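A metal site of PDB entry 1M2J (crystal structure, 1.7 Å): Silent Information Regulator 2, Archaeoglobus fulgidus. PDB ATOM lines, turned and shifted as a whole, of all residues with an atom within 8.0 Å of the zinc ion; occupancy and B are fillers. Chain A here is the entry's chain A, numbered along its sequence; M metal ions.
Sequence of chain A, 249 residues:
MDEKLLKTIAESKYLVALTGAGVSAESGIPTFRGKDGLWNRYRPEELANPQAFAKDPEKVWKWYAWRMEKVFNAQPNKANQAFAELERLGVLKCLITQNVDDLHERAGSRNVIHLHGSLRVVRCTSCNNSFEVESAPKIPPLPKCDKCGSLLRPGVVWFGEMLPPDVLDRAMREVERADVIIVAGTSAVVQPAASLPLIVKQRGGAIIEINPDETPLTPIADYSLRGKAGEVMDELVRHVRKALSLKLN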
ATOM      1  N   ARG A 123     -22.630 -33.899 -16.985  1.00  0.00           N
ATOM      2  CA  ARG A 123     -22.404 -32.507 -17.341  1.00  0.00           C
ATOM      3  C   ARG A 123     -21.485 -31.789 -16.374  1.00  0.00           C
ATOM      4  O   ARG A 123     -21.305 -32.225 -15.235  1.00  0.00           O
ATOM      5  CB  ARG A 123     -23.739 -31.747 -17.440  1.00  0.00           C
ATOM      6  CG  ARG A 123     -24.451 -31.512 -16.119  1.00  0.00           C
ATOM      7  CD  ARG A 123     -25.784 -30.797 -16.368  1.00  0.00           C
ATOM      8  NE  ARG A 123     -26.542 -30.534 -15.149  1.00  0.00           N
ATOM      9  CZ  ARG A 123     -26.216 -29.631 -14.235  1.00  0.00           C
ATOM     10  NH1 ARG A 123     -25.124 -28.888 -14.385  1.00  0.00           N
ATOM     11  NH2 ARG A 123     -26.988 -29.453 -13.173  1.00  0.00           N
ATOM     12  N   CYS A 124     -20.902 -30.697 -16.841  1.00  0.00           N
ATOM     13  CA  CYS A 124     -19.988 -29.924 -16.034  1.00  0.00           C
ATOM     14  C   CYS A 124     -20.708 -29.038 -15.039  1.00  0.00           C
ATOM     15  O   CYS A 124     -21.803 -28.544 -15.323  1.00  0.00           O
ATOM     16  CB  CYS A 124     -19.106 -29.065 -16.933  1.00  0.00           C
ATOM     17  SG  CYS A 124     -17.839 -28.145 -16.012  1.00  0.00           S
ATOM     18  N   THR A 125     -20.100 -28.844 -13.876  1.00  0.00           N
ATOM     19  CA  THR A 125     -20.690 -28.013 -12.840  1.00  0.00           C
ATOM     20  C   THR A 125     -20.367 -26.534 -13.082  1.00  0.00           C
ATOM     21  O   THR A 125     -20.941 -25.661 -12.442  1.00  0.00           O
ATOM     22  CB  THR A 125     -20.170 -28.405 -11.441  1.00  0.00           C
ATOM     23  OG1 THR A 125     -18.742 -28.306 -11.423  1.00  0.00           O
ATOM     24  CG2 THR A 125     -20.586 -29.823 -11.094  1.00  0.00           C
ATOM     25  N   SER A 126     -19.446 -26.276 -14.017  1.00  0.00           N
ATOM     26  CA  SER A 126     -19.047 -24.906 -14.326  1.00  0.00           C
ATOM     27  C   SER A 126     -19.482 -24.426 -15.711  1.00  0.00           C
ATOM     28  O   SER A 126     -20.294 -23.512 -15.827  1.00  0.00           O
ATOM     29  CB  SER A 126     -17.525 -24.760 -14.208  1.00  0.00           C
ATOM     30  OG  SER A 126     -17.096 -24.989 -12.878  1.00  0.00           O
ATOM     31  N   CYS A 127     -18.931 -25.040 -16.757  1.00  0.00           N
ATOM     32  CA  CYS A 127     -19.287 -24.637 -18.114  1.00  0.00           C
ATOM     33  C   CYS A 127     -20.482 -25.445 -18.627  1.00  0.00           C
ATOM     34  O   CYS A 127     -21.095 -26.197 -17.868  1.00  0.00           O
ATOM     35  CB  CYS A 127     -18.084 -24.807 -19.055  1.00  0.00           C
ATOM     36  SG  CYS A 127     -17.625 -26.517 -19.458  1.00  0.00           S
ATOM     37  N   ASN A 128     -20.799 -25.293 -19.912  1.00  0.00           N
ATOM     38  CA  ASN A 128     -21.953 -25.982 -20.483  1.00  0.00           C
ATOM     39  C   ASN A 128     -21.648 -27.337 -21.110  1.00  0.00           C
ATOM     40  O   ASN A 128     -22.483 -27.899 -21.821  1.00  0.00           O
ATOM     41  CB  ASN A 128     -22.631 -25.076 -21.514  1.00  0.00           C
ATOM     42  CG  ASN A 128     -24.025 -25.559 -21.890  1.00  0.00           C
ATOM     43  OD1 ASN A 128     -24.904 -25.695 -21.035  1.00  0.00           O
ATOM     44  ND2 ASN A 128     -24.237 -25.825 -23.173  1.00  0.00           N
ATOM     45  N   ASN A 129     -20.464 -27.875 -20.848  1.00  0.00           N
ATOM     46  CA  ASN A 129     -20.103 -29.169 -21.411  1.00  0.00           C
ATOM     47  C   ASN A 129     -21.015 -30.265 -20.859  1.00  0.00           C
ATOM     48  O   ASN A 129     -21.257 -30.341 -19.656  1.00  0.00           O
ATOM     49  CB  ASN A 129     -18.644 -29.510 -21.081  1.00  0.00           C
ATOM     50  CG  ASN A 129     -18.169 -30.773 -21.794  1.00  0.00           C
ATOM     51  OD1 ASN A 129     -17.098 -31.301 -21.488  1.00  0.00           O
ATOM     52  ND2 ASN A 129     -18.947 -31.244 -22.761  1.00  0.00           N
ATOM     53  N   SER A 130     -21.527 -31.099 -21.755  1.00  0.00           N
ATOM     54  CA  SER A 130     -22.395 -32.210 -21.362  1.00  0.00           C
ATOM     55  C   SER A 130     -22.241 -33.276 -22.440  1.00  0.00           C
ATOM     56  O   SER A 130     -21.926 -32.972 -23.585  1.00  0.00           O
ATOM     57  CB  SER A 130     -23.858 -31.763 -21.257  1.00  0.00           C
ATOM     58  OG  SER A 130     -24.380 -31.414 -22.527  1.00  0.00           O
ATOM     59  N   LYS A 144     -13.638 -35.299 -14.207  1.00  0.00           N
ATOM     60  CA  LYS A 144     -13.353 -33.899 -14.447  1.00  0.00           C
ATOM     61  C   LYS A 144     -13.616 -33.497 -15.883  1.00  0.00           C
ATOM     62  O   LYS A 144     -13.370 -34.258 -16.823  1.00  0.00           O
ATOM     63  CB  LYS A 144     -11.908 -33.573 -14.042  1.00  0.00           C
ATOM     64  CG  LYS A 144     -11.658 -33.746 -12.555  1.00  0.00           C
ATOM     65  CD  LYS A 144     -10.257 -33.307 -12.158  1.00  0.00           C
ATOM     66  CE  LYS A 144     -10.039 -33.452 -10.658  1.00  0.00           C
ATOM     67  NZ  LYS A 144     -11.043 -32.660  -9.884  1.00  0.00           N
ATOM     68  N   CYS A 145     -14.116 -32.276 -16.044  1.00  0.00           N
ATOM     69  CA  CYS A 145     -14.434 -31.714 -17.337  1.00  0.00           C
ATOM     70  C   CYS A 145     -13.192 -31.540 -18.199  1.00  0.00           C
ATOM     71  O   CYS A 145     -12.192 -30.975 -17.768  1.00  0.00           O
ATOM     72  CB  CYS A 145     -15.127 -30.372 -17.143  1.00  0.00           C
ATOM     73  SG  CYS A 145     -15.596 -29.561 -18.692  1.00  0.00           S
ATOM     74  N   ASP A 146     -13.267 -32.021 -19.438  1.00  0.00           N
ATOM     75  CA  ASP A 146     -12.152 -31.930 -20.370  1.00  0.00           C
ATOM     76  C   ASP A 146     -12.052 -30.545 -21.001  1.00  0.00           C
ATOM     77  O   ASP A 146     -11.101 -30.247 -21.709  1.00  0.00           O
ATOM     78  CB  ASP A 146     -12.297 -33.000 -21.466  1.00  0.00           C
ATOM     79  CG  ASP A 146     -13.543 -32.801 -22.308  1.00  0.00           C
ATOM     80  OD1 ASP A 146     -13.583 -31.823 -23.093  1.00  0.00           O
ATOM     81  OD2 ASP A 146     -14.489 -33.607 -22.181  1.00  0.00           O
ATOM     82  N   LYS A 147     -13.036 -29.694 -20.720  1.00  0.00           N
ATOM     83  CA  LYS A 147     -13.056 -28.350 -21.270  1.00  0.00           C
ATOM     84  C   LYS A 147     -12.463 -27.296 -20.345  1.00  0.00           C
ATOM     85  O   LYS A 147     -11.687 -26.436 -20.790  1.00  0.00           O
ATOM     86  CB  LYS A 147     -14.482 -27.946 -21.649  1.00  0.00           C
ATOM     87  CG  LYS A 147     -15.110 -28.792 -22.749  1.00  0.00           C
ATOM     88  CD  LYS A 147     -14.285 -28.745 -24.016  1.00  0.00           C
ATOM     89  CE  LYS A 147     -14.865 -29.635 -25.098  1.00  0.00           C
ATOM     90  NZ  LYS A 147     -14.029 -29.623 -26.325  1.00  0.00           N
ATOM     91  N   CYS A 148     -12.812 -27.349 -19.065  1.00  0.00           N
ATOM     92  CA  CYS A 148     -12.308 -26.365 -18.107  1.00  0.00           C
ATOM     93  C   CYS A 148     -11.670 -26.982 -16.868  1.00  0.00           C
ATOM     94  O   CYS A 148     -11.097 -26.272 -16.030  1.00  0.00           O
ATOM     95  CB  CYS A 148     -13.438 -25.428 -17.690  1.00  0.00           C
ATOM     96  SG  CYS A 148     -14.789 -26.287 -16.832  1.00  0.00           S
ATOM     97  N   GLY A 149     -11.781 -28.304 -16.734  1.00  0.00           N
ATOM     98  CA  GLY A 149     -11.185 -28.971 -15.598  1.00  0.00           C
ATOM     99  C   GLY A 149     -11.997 -29.012 -14.311  1.00  0.00           C
ATOM    100  O   GLY A 149     -11.538 -29.574 -13.318  1.00  0.00           O
ATOM    101  N   SER A 150     -13.176 -28.417 -14.303  1.00  0.00           N
ATOM    102  CA  SER A 150     -13.994 -28.439 -13.090  1.00  0.00           C
ATOM    103  C   SER A 150     -14.675 -29.783 -12.934  1.00  0.00           C
ATOM    104  O   SER A 150     -14.667 -30.615 -13.851  1.00  0.00           O
ATOM    105  CB  SER A 150     -15.036 -27.314 -13.127  1.00  0.00           C
ATOM    106  OG  SER A 150     -15.792 -27.354 -14.316  1.00  0.00           O
ATOM    107  N   LEU A 151     -15.253 -30.020 -11.764  1.00  0.00           N
ATOM    108  CA  LEU A 151     -15.927 -31.293 -11.499  1.00  0.00           C
ATOM    109  C   LEU A 151     -17.149 -31.529 -12.381  1.00  0.00           C
ATOM    110  O   LEU A 151     -17.909 -30.606 -12.675  1.00  0.00           O
ATOM    111  CB  LEU A 151     -16.382 -31.357 -10.029  1.00  0.00           C
ATOM    112  CG  LEU A 151     -15.326 -31.541  -8.936  1.00  0.00           C
ATOM    113  CD1 LEU A 151     -16.018 -31.605  -7.591  1.00  0.00           C
ATOM    114  CD2 LEU A 151     -14.524 -32.811  -9.194  1.00  0.00           C
ATOM    115  N   LEU A 152     -17.311 -32.779 -12.807  1.00  0.00           N
ATOM    116  CA  LEU A 152     -18.464 -33.154 -13.609  1.00  0.00           C
ATOM    117  C   LEU A 152     -19.478 -33.705 -12.619  1.00  0.00           C
ATOM    118  O   LEU A 152     -19.115 -34.014 -11.478  1.00  0.00           O
ATOM    119  CB  LEU A 152     -18.095 -34.246 -14.621  1.00  0.00           C
ATOM    120  CG  LEU A 152     -17.239 -33.854 -15.824  1.00  0.00           C
ATOM    121  CD1 LEU A 152     -16.846 -35.105 -16.583  1.00  0.00           C
ATOM    122  CD2 LEU A 152     -18.013 -32.901 -16.711  1.00  0.00           C
HETATM  123 ZN    ZN M   1     -16.454 -27.604 -17.771  1.00  0.00          ZN
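The zinc ion is bound by SG of Cys 124 (2.3 Å), SG of Cys 148 (2.3 Å), SG of Cys 127 (2.3 Å) and SG of Cys 145 (2.3 Å).
Residues that only touch the zinc ion: Ser 150. Five residues have an atom within 4 Å of the zinc ion: Cys 124, Cys 127, Cys 145, Cys 148 and Ser 150.
The side-chain sulfur of Cys 127 lies close to the backbone NH of Asn 129 (3.4 Å). The side-chain sulfur of Cys 124 lies close to the backbone NH of Ser 126. The backbone NH of Cys 145 is in hydrogen-bond range of the backbone carbonyl oxygen of Ser 150 (2.8 Å). SG of Cys 124 sits close to OG of Ser 150, 2.8 Å away. OG of Ser 150 lies within hydrogen-bond range of OG of Ser 126. The backbone carbonyl oxygen (O) of Asn 129 is in hydrogen-bond range of the backbone NH (N) of Cys 124 (2.9 Å). SG of Cys 145 sits close to OD1 of Asn 129. SG of Cys 148 lies close to OG of Ser 150 (2.9 Å).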
